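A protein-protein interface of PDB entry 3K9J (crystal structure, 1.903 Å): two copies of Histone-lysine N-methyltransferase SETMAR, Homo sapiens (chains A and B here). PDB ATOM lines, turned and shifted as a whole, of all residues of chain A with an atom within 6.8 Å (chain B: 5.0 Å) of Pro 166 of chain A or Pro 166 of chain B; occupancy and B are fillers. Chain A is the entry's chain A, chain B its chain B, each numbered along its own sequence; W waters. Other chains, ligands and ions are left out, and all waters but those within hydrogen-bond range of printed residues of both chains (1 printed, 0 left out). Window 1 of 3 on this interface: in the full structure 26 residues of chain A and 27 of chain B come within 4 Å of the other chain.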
ATOM      1  N   GLU A  29      27.501  24.429 -32.335  1.00  0.00           N
ATOM      2  CA  GLU A  29      27.794  23.374 -31.368  1.00  0.00           C
ATOM      3  C   GLU A  29      26.523  22.706 -30.812  1.00  0.00           C
ATOM      4  O   GLU A  29      26.368  21.491 -30.862  1.00  0.00           O
ATOM      5  CB  GLU A  29      28.615  23.961 -30.211  1.00  0.00           C
ATOM      6  CG  GLU A  29      29.050  22.957 -29.177  1.00  0.00           C
ATOM      7  CD  GLU A  29      29.742  23.616 -27.990  1.00  0.00           C
ATOM      8  OE1 GLU A  29      30.919  24.015 -28.126  1.00  0.00           O
ATOM      9  OE2 GLU A  29      29.106  23.728 -26.920  1.00  0.00           O
ATOM     10  N   VAL A  30      25.624  23.513 -30.279  1.00  0.00           N
ATOM     11  CA  VAL A  30      24.407  22.987 -29.660  1.00  0.00           C
ATOM     12  C   VAL A  30      23.471  22.319 -30.677  1.00  0.00           C
ATOM     13  O   VAL A  30      22.989  21.204 -30.438  1.00  0.00           O
ATOM     14  CB  VAL A  30      23.658  24.079 -28.864  1.00  0.00           C
ATOM     15  CG1 VAL A  30      22.285  23.562 -28.374  1.00  0.00           C
ATOM     16  CG2 VAL A  30      24.506  24.590 -27.693  1.00  0.00           C
ATOM     17  N   SER A  33      24.878  18.937 -31.769  1.00  0.00           N
ATOM     18  CA  SER A  33      24.746  17.919 -30.735  1.00  0.00           C
ATOM     19  C   SER A  33      23.287  17.480 -30.542  1.00  0.00           C
ATOM     20  O   SER A  33      23.033  16.310 -30.300  1.00  0.00           O
ATOM     21  CB  SER A  33      25.345  18.389 -29.400  1.00  0.00           C
ATOM     22  OG  SER A  33      26.773  18.355 -29.471  1.00  0.00           O
ATOM     23  N   LEU A  34      22.347  18.413 -30.624  1.00  0.00           N
ATOM     24  CA  LEU A  34      20.923  18.053 -30.519  1.00  0.00           C
ATOM     25  C   LEU A  34      20.457  17.153 -31.664  1.00  0.00           C
ATOM     26  O   LEU A  34      19.714  16.186 -31.442  1.00  0.00           O
ATOM     27  CB  LEU A  34      20.038  19.295 -30.416  1.00  0.00           C
ATOM     28  CG  LEU A  34      20.258  20.111 -29.145  1.00  0.00           C
ATOM     29  CD1 LEU A  34      19.456  21.398 -29.181  1.00  0.00           C
ATOM     30  CD2 LEU A  34      19.873  19.289 -27.923  1.00  0.00           C
ATOM     31  N   ARG A  37      22.072  13.772 -30.946  1.00  0.00           N
ATOM     32  CA  ARG A  37      21.469  13.183 -29.767  1.00  0.00           C
ATOM     33  C   ARG A  37      20.121  12.587 -30.133  1.00  0.00           C
ATOM     34  O   ARG A  37      19.799  11.453 -29.768  1.00  0.00           O
ATOM     35  CB  ARG A  37      21.287  14.243 -28.689  1.00  0.00           C
ATOM     36  CG  ARG A  37      20.555  13.706 -27.461  1.00  0.00           C
ATOM     37  CD  ARG A  37      20.458  14.727 -26.355  1.00  0.00           C
ATOM     38  NE  ARG A  37      19.665  14.213 -25.242  1.00  0.00           N
ATOM     39  CZ  ARG A  37      19.464  14.862 -24.106  1.00  0.00           C
ATOM     40  NH1 ARG A  37      20.009  16.056 -23.906  1.00  0.00           N
ATOM     41  NH2 ARG A  37      18.715  14.305 -23.175  1.00  0.00           N
ATOM     42  N   ILE A 139      11.738  16.796 -20.605  1.00  0.00           N
ATOM     43  CA  ILE A 139      12.914  17.651 -20.769  1.00  0.00           C
ATOM     44  C   ILE A 139      12.451  19.072 -21.082  1.00  0.00           C
ATOM     45  O   ILE A 139      11.641  19.281 -21.989  1.00  0.00           O
ATOM     46  CB  ILE A 139      13.761  17.165 -21.944  1.00  0.00           C
ATOM     47  CG1 ILE A 139      14.250  15.738 -21.693  1.00  0.00           C
ATOM     48  CG2 ILE A 139      14.937  18.105 -22.206  1.00  0.00           C
ATOM     49  CD1 ILE A 139      14.883  15.108 -22.944  1.00  0.00           C
ATOM     50  N   LEU A 140      12.969  20.051 -20.353  1.00  0.00           N
ATOM     51  CA  LEU A 140      12.538  21.430 -20.548  1.00  0.00           C
ATOM     52  C   LEU A 140      13.394  22.103 -21.590  1.00  0.00           C
ATOM     53  O   LEU A 140      14.617  22.027 -21.534  1.00  0.00           O
ATOM     54  CB  LEU A 140      12.634  22.238 -19.252  1.00  0.00           C
ATOM     55  CG  LEU A 140      12.077  23.673 -19.338  1.00  0.00           C
ATOM     56  CD1 LEU A 140      10.578  23.656 -19.632  1.00  0.00           C
ATOM     57  CD2 LEU A 140      12.361  24.496 -18.071  1.00  0.00           C
ATOM     58  N   LEU A 141      12.748  22.765 -22.543  1.00  0.00           N
ATOM     59  CA  LEU A 141      13.468  23.586 -23.505  1.00  0.00           C
ATOM     60  C   LEU A 141      12.963  25.001 -23.282  1.00  0.00           C
ATOM     61  O   LEU A 141      11.797  25.303 -23.521  1.00  0.00           O
ATOM     62  CB  LEU A 141      13.158  23.132 -24.925  1.00  0.00           C
ATOM     63  CG  LEU A 141      13.601  24.060 -26.058  1.00  0.00           C
ATOM     64  CD1 LEU A 141      15.054  24.425 -25.894  1.00  0.00           C
ATOM     65  CD2 LEU A 141      13.348  23.398 -27.391  1.00  0.00           C
ATOM     66  N   HIS A 142      13.825  25.858 -22.761  1.00  0.00           N
ATOM     67  CA  HIS A 142      13.454  27.251 -22.558  1.00  0.00           C
ATOM     68  C   HIS A 142      14.676  28.108 -22.743  1.00  0.00           C
ATOM     69  O   HIS A 142      15.790  27.587 -22.868  1.00  0.00           O
ATOM     70  CB  HIS A 142      12.757  27.476 -21.198  1.00  0.00           C
ATOM     71  CG  HIS A 142      13.661  27.389 -20.002  1.00  0.00           C
ATOM     72  ND1 HIS A 142      14.907  26.802 -20.039  1.00  0.00           N
ATOM     73  CD2 HIS A 142      13.463  27.770 -18.719  1.00  0.00           C
ATOM     74  CE1 HIS A 142      15.455  26.858 -18.833  1.00  0.00           C
ATOM     75  NE2 HIS A 142      14.596  27.439 -18.017  1.00  0.00           N
ATOM     76  N   ASN A 144      17.446  31.439 -22.082  1.00  0.00           N
ATOM     77  CA  ASN A 144      18.352  31.838 -21.004  1.00  0.00           C
ATOM     78  C   ASN A 144      17.992  33.186 -20.373  1.00  0.00           C
ATOM     79  O   ASN A 144      18.841  33.836 -19.769  1.00  0.00           O
ATOM     80  CB  ASN A 144      19.788  31.856 -21.526  1.00  0.00           C
ATOM     81  CG  ASN A 144      20.200  30.516 -22.151  1.00  0.00           C
ATOM     82  OD1 ASN A 144      20.401  30.406 -23.377  1.00  0.00           O
ATOM     83  ND2 ASN A 144      20.329  29.488 -21.304  1.00  0.00           N
ATOM     84  N   GLU A 163      15.330  17.434 -16.623  1.00  0.00           N
ATOM     85  CA  GLU A 163      16.529  17.708 -17.381  1.00  0.00           C
ATOM     86  C   GLU A 163      16.234  18.965 -18.214  1.00  0.00           C
ATOM     87  O   GLU A 163      15.118  19.138 -18.692  1.00  0.00           O
ATOM     88  CB  GLU A 163      16.768  16.494 -18.276  1.00  0.00           C
ATOM     89  CG  GLU A 163      18.097  16.394 -18.898  1.00  0.00           C
ATOM     90  CD  GLU A 163      18.089  15.401 -20.050  1.00  0.00           C
ATOM     91  OE1 GLU A 163      17.405  14.345 -19.977  1.00  0.00           O
ATOM     92  OE2 GLU A 163      18.773  15.690 -21.013  1.00  0.00           O
ATOM     93  N   VAL A 164      17.201  19.861 -18.365  1.00  0.00           N
ATOM     94  CA  VAL A 164      17.020  21.015 -19.242  1.00  0.00           C
ATOM     95  C   VAL A 164      17.889  20.866 -20.509  1.00  0.00           C
ATOM     96  O   VAL A 164      19.080  20.624 -20.401  1.00  0.00           O
ATOM     97  CB  VAL A 164      17.395  22.325 -18.513  1.00  0.00           C
ATOM     98  CG1 VAL A 164      17.208  23.521 -19.434  1.00  0.00           C
ATOM     99  CG2 VAL A 164      16.551  22.503 -17.251  1.00  0.00           C
ATOM    100  N   LEU A 165      17.304  21.024 -21.697  1.00  0.00           N
ATOM    101  CA  LEU A 165      18.068  20.937 -22.960  1.00  0.00           C
ATOM    102  C   LEU A 165      19.042  22.120 -23.127  1.00  0.00           C
ATOM    103  O   LEU A 165      18.708  23.251 -22.777  1.00  0.00           O
ATOM    104  CB  LEU A 165      17.079  20.906 -24.141  1.00  0.00           C
ATOM    105  CG  LEU A 165      17.318  20.114 -25.422  1.00  0.00           C
ATOM    106  CD1 LEU A 165      17.622  18.646 -25.139  1.00  0.00           C
ATOM    107  CD2 LEU A 165      16.111  20.264 -26.362  1.00  0.00           C
ATOM    108  N   PRO A 166      20.259  21.870 -23.658  1.00  0.00           N
ATOM    109  CA  PRO A 166      21.144  22.988 -23.997  1.00  0.00           C
ATOM    110  C   PRO A 166      20.479  23.933 -24.979  1.00  0.00           C
ATOM    111  O   PRO A 166      19.787  23.488 -25.887  1.00  0.00           O
ATOM    112  CB  PRO A 166      22.330  22.309 -24.699  1.00  0.00           C
ATOM    113  CG  PRO A 166      22.300  20.917 -24.254  1.00  0.00           C
ATOM    114  CD  PRO A 166      20.864  20.569 -23.994  1.00  0.00           C
ATOM    115  N   HIS A 167      20.673  25.227 -24.789  1.00  0.00           N
ATOM    116  CA  HIS A 167      20.127  26.209 -25.711  1.00  0.00           C
ATOM    117  C   HIS A 167      21.135  27.346 -25.839  1.00  0.00           C
ATOM    118  O   HIS A 167      21.542  27.915 -24.837  1.00  0.00           O
ATOM    119  CB  HIS A 167      18.766  26.737 -25.224  1.00  0.00           C
ATOM    120  CG  HIS A 167      18.152  27.732 -26.157  1.00  0.00           C
ATOM    121  ND1 HIS A 167      17.614  27.368 -27.372  1.00  0.00           N
ATOM    122  CD2 HIS A 167      18.034  29.074 -26.077  1.00  0.00           C
ATOM    123  CE1 HIS A 167      17.178  28.448 -27.998  1.00  0.00           C
ATOM    124  NE2 HIS A 167      17.410  29.498 -27.223  1.00  0.00           N
ATOM    125  N   PRO A 168      21.558  27.661 -27.076  1.00  0.00           N
ATOM    126  CA  PRO A 168      22.537  28.731 -27.275  1.00  0.00           C
ATOM    127  C   PRO A 168      21.856  30.095 -27.193  1.00  0.00           C
ATOM    128  O   PRO A 168      20.687  30.204 -27.565  1.00  0.00           O
ATOM    129  CB  PRO A 168      23.027  28.454 -28.698  1.00  0.00           C
ATOM    130  CG  PRO A 168      21.755  28.050 -29.396  1.00  0.00           C
ATOM    131  CD  PRO A 168      21.102  27.109 -28.371  1.00  0.00           C
ATOM    132  N   TRP A 227      17.540  22.939 -36.422  1.00  0.00           N
ATOM    133  CA  TRP A 227      18.916  22.584 -36.041  1.00  0.00           C
ATOM    134  C   TRP A 227      19.786  22.362 -37.274  1.00  0.00           C
ATOM    135  O   TRP A 227      20.939  22.821 -37.315  1.00  0.00           O
ATOM    136  CB  TRP A 227      18.992  21.341 -35.149  1.00  0.00           C
ATOM    137  CG  TRP A 227      18.277  21.489 -33.828  1.00  0.00           C
ATOM    138  CD1 TRP A 227      18.123  22.633 -33.099  1.00  0.00           C
ATOM    139  CD2 TRP A 227      17.624  20.454 -33.096  1.00  0.00           C
ATOM    140  NE1 TRP A 227      17.409  22.374 -31.949  1.00  0.00           N
ATOM    141  CE2 TRP A 227      17.089  21.041 -31.925  1.00  0.00           C
ATOM    142  CE3 TRP A 227      17.439  19.088 -33.311  1.00  0.00           C
ATOM    143  CZ2 TRP A 227      16.370  20.308 -30.974  1.00  0.00           C
ATOM    144  CZ3 TRP A 227      16.700  18.359 -32.356  1.00  0.00           C
ATOM    145  CH2 TRP A 227      16.199  18.971 -31.205  1.00  0.00           C
ATOM    146  N   VAL B  30      23.800  22.700 -15.382  1.00  0.00           N
ATOM    147  CA  VAL B  30      24.418  21.628 -16.141  1.00  0.00           C
ATOM    148  C   VAL B  30      24.593  20.371 -15.310  1.00  0.00           C
ATOM    149  O   VAL B  30      24.277  19.273 -15.768  1.00  0.00           O
ATOM    150  CB  VAL B  30      25.782  22.067 -16.725  1.00  0.00           C
ATOM    151  CG1 VAL B  30      26.441  20.903 -17.455  1.00  0.00           C
ATOM    152  CG2 VAL B  30      25.601  23.278 -17.655  1.00  0.00           C
ATOM    153  N   LEU B  34      22.815  16.860 -16.252  1.00  0.00           N
ATOM    154  CA  LEU B  34      23.605  15.660 -16.539  1.00  0.00           C
ATOM    155  C   LEU B  34      23.273  14.451 -15.667  1.00  0.00           C
ATOM    156  O   LEU B  34      23.215  13.319 -16.152  1.00  0.00           O
ATOM    157  CB  LEU B  34      25.097  15.968 -16.488  1.00  0.00           C
ATOM    158  CG  LEU B  34      25.545  16.932 -17.593  1.00  0.00           C
ATOM    159  CD1 LEU B  34      26.972  17.335 -17.377  1.00  0.00           C
ATOM    160  CD2 LEU B  34      25.340  16.325 -18.991  1.00  0.00           C
ATOM    161  N   ARG B  37      19.903  13.330 -16.936  1.00  0.00           N
ATOM    162  CA  ARG B  37      20.041  12.689 -18.233  1.00  0.00           C
ATOM    163  C   ARG B  37      20.589  11.268 -18.074  1.00  0.00           C
ATOM    164  O   ARG B  37      20.082  10.334 -18.689  1.00  0.00           O
ATOM    165  CB  ARG B  37      20.931  13.517 -19.164  1.00  0.00           C
ATOM    166  CG  ARG B  37      21.209  12.786 -20.468  1.00  0.00           C
ATOM    167  CD  ARG B  37      22.028  13.627 -21.447  1.00  0.00           C
ATOM    168  NE  ARG B  37      22.271  12.862 -22.666  1.00  0.00           N
ATOM    169  CZ  ARG B  37      22.969  13.299 -23.710  1.00  0.00           C
ATOM    170  NH1 ARG B  37      23.431  14.539 -23.733  1.00  0.00           N
ATOM    171  NH2 ARG B  37      23.149  12.505 -24.757  1.00  0.00           N
ATOM    172  N   LEU B 141      33.339  14.985 -23.894  1.00  0.00           N
ATOM    173  CA  LEU B 141      33.354  15.923 -22.782  1.00  0.00           C
ATOM    174  C   LEU B 141      34.682  16.665 -22.857  1.00  0.00           C
ATOM    175  O   LEU B 141      35.747  16.054 -22.748  1.00  0.00           O
ATOM    176  CB  LEU B 141      33.255  15.156 -21.456  1.00  0.00           C
ATOM    177  CG  LEU B 141      33.430  15.902 -20.131  1.00  0.00           C
ATOM    178  CD1 LEU B 141      32.597  17.152 -20.126  1.00  0.00           C
ATOM    179  CD2 LEU B 141      33.037  15.007 -18.967  1.00  0.00           C
ATOM    180  N   VAL B 164      28.471  16.498 -28.194  1.00  0.00           N
ATOM    181  CA  VAL B 164      29.305  17.116 -27.154  1.00  0.00           C
ATOM    182  C   VAL B 164      28.436  17.377 -25.920  1.00  0.00           C
ATOM    183  O   VAL B 164      27.295  17.791 -26.038  1.00  0.00           O
ATOM    184  CB  VAL B 164      29.985  18.436 -27.635  1.00  0.00           C
ATOM    185  CG1 VAL B 164      30.798  19.081 -26.525  1.00  0.00           C
ATOM    186  CG2 VAL B 164      30.913  18.171 -28.829  1.00  0.00           C
ATOM    187  N   LEU B 165      28.974  17.117 -24.737  1.00  0.00           N
ATOM    188  CA  LEU B 165      28.207  17.273 -23.512  1.00  0.00           C
ATOM    189  C   LEU B 165      28.295  18.739 -23.085  1.00  0.00           C
ATOM    190  O   LEU B 165      29.326  19.377 -23.255  1.00  0.00           O
ATOM    191  CB  LEU B 165      28.832  16.366 -22.443  1.00  0.00           C
ATOM    192  CG  LEU B 165      28.074  15.538 -21.418  1.00  0.00           C
ATOM    193  CD1 LEU B 165      26.861  14.812 -21.994  1.00  0.00           C
ATOM    194  CD2 LEU B 165      29.060  14.539 -20.822  1.00  0.00           C
ATOM    195  N   PRO B 166      27.203  19.291 -22.577  1.00  0.00           N
ATOM    196  CA  PRO B 166      27.205  20.637 -21.992  1.00  0.00           C
ATOM    197  C   PRO B 166      28.281  20.699 -20.911  1.00  0.00           C
ATOM    198  O   PRO B 166      28.464  19.702 -20.235  1.00  0.00           O
ATOM    199  CB  PRO B 166      25.822  20.720 -21.329  1.00  0.00           C
ATOM    200  CG  PRO B 166      24.970  19.828 -22.164  1.00  0.00           C
ATOM    201  CD  PRO B 166      25.839  18.725 -22.683  1.00  0.00           C
ATOM    202  N   HIS B 167      28.961  21.829 -20.756  1.00  0.00           N
ATOM    203  CA  HIS B 167      29.983  21.989 -19.710  1.00  0.00           C
ATOM    204  C   HIS B 167      30.034  23.444 -19.269  1.00  0.00           C
ATOM    205  O   HIS B 167      30.236  24.323 -20.094  1.00  0.00           O
ATOM    206  CB  HIS B 167      31.371  21.576 -20.224  1.00  0.00           C
ATOM    207  CG  HIS B 167      32.453  21.695 -19.189  1.00  0.00           C
ATOM    208  ND1 HIS B 167      32.534  20.852 -18.101  1.00  0.00           N
ATOM    209  CD2 HIS B 167      33.480  22.570 -19.062  1.00  0.00           C
ATOM    210  CE1 HIS B 167      33.572  21.195 -17.353  1.00  0.00           C
ATOM    211  NE2 HIS B 167      34.165  22.235 -17.916  1.00  0.00           N
ATOM    212  N   PRO B 168      29.880  23.706 -17.960  1.00  0.00           N
ATOM    213  CA  PRO B 168      29.862  25.104 -17.525  1.00  0.00           C
ATOM    214  C   PRO B 168      31.271  25.676 -17.447  1.00  0.00           C
ATOM    215  O   PRO B 168      32.216  24.919 -17.238  1.00  0.00           O
ATOM    216  CB  PRO B 168      29.295  25.026 -16.108  1.00  0.00           C
ATOM    217  CG  PRO B 168      29.492  23.586 -15.668  1.00  0.00           C
ATOM    218  CD  PRO B 168      29.931  22.762 -16.831  1.00  0.00           C
HETATM  219  O   HOH W   1      29.786  22.097 -24.332  1.00  0.00           O
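The backbone NH (N) of Val 164 of chain B lies within hydrogen-bond range of the side-chain hydroxyl (OG) of Ser 33 of chain A (2.8 Å).
Arg 37 of chain B touches its own counterpart, Arg 37 of chain A. Pro 166 of chain A touches its own counterpart, Pro 166 of chain B. 9 positions are printed for both chains.
Glu 29 of chain A touches none of the printed residues of chain B. Of the printed residues of chain B, Ser 33 of chain A touches Val 164 (2.8 Å). Of the printed residues of chain B, Arg 37 of chain A touches Arg 37 (3.7 Å). Printed residues of chain B within 4 Å of Glu 163 of chain A: Arg 37 (3.5 Å). Of the printed residues of chain A, Arg 37 of chain B touches Arg 37 (3.7 Å) and Glu 163 (3.5 Å). Printed residues of chain A within 4 Å of Val 164 of chain B: Ser 33. Pro 166 of chain B touches just one residue of chain A: Pro 166. The nearest printed residue of chain A that does not touch Val 164 of chain B is Glu 29 of chain A (4.9 Å).
Among the printed residues, pairs that only touch across the chains: Glu 163 of chain A with Arg 37 of chain B (3.5 Å), Pro 166 of chain A with Pro 166 of chain B (3.6 Å) and Arg 37 of chain A with Arg 37 of chain B (3.7 Å).
Water W1 bridges the backbone carbonyl oxygen (O) of Leu 165 of chain B (3.0 Å) and the side-chain carboxylate (OE2) of Glu 29 of chain A (3.1 Å).
Hydrophobic or aromatic side chains of chain B within 4 Å of the printed part of chain A: Val 164 and Pro 166. Hydrophobic or aromatic side chains of chain A within 4 Å of the printed part of chain B: Pro 166. Among the printed residues, no Asp or Glu carboxylate lies within 4 Å of a Lys or Arg side-chain nitrogen of the other chain.
OG of Ser 33 of chain A sits at hydrogen-bond distance from O of Glu 29 of chain A (3.5 Å). N of Leu 140 of chain A lies within hydrogen-bond range of O of Glu 163 of chain A (2.9 Å). The guanidinium group of Arg 37 of chain A lies within salt-bridge range of the side-chain carboxylate of Glu 163 of chain A (2.6 Å).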
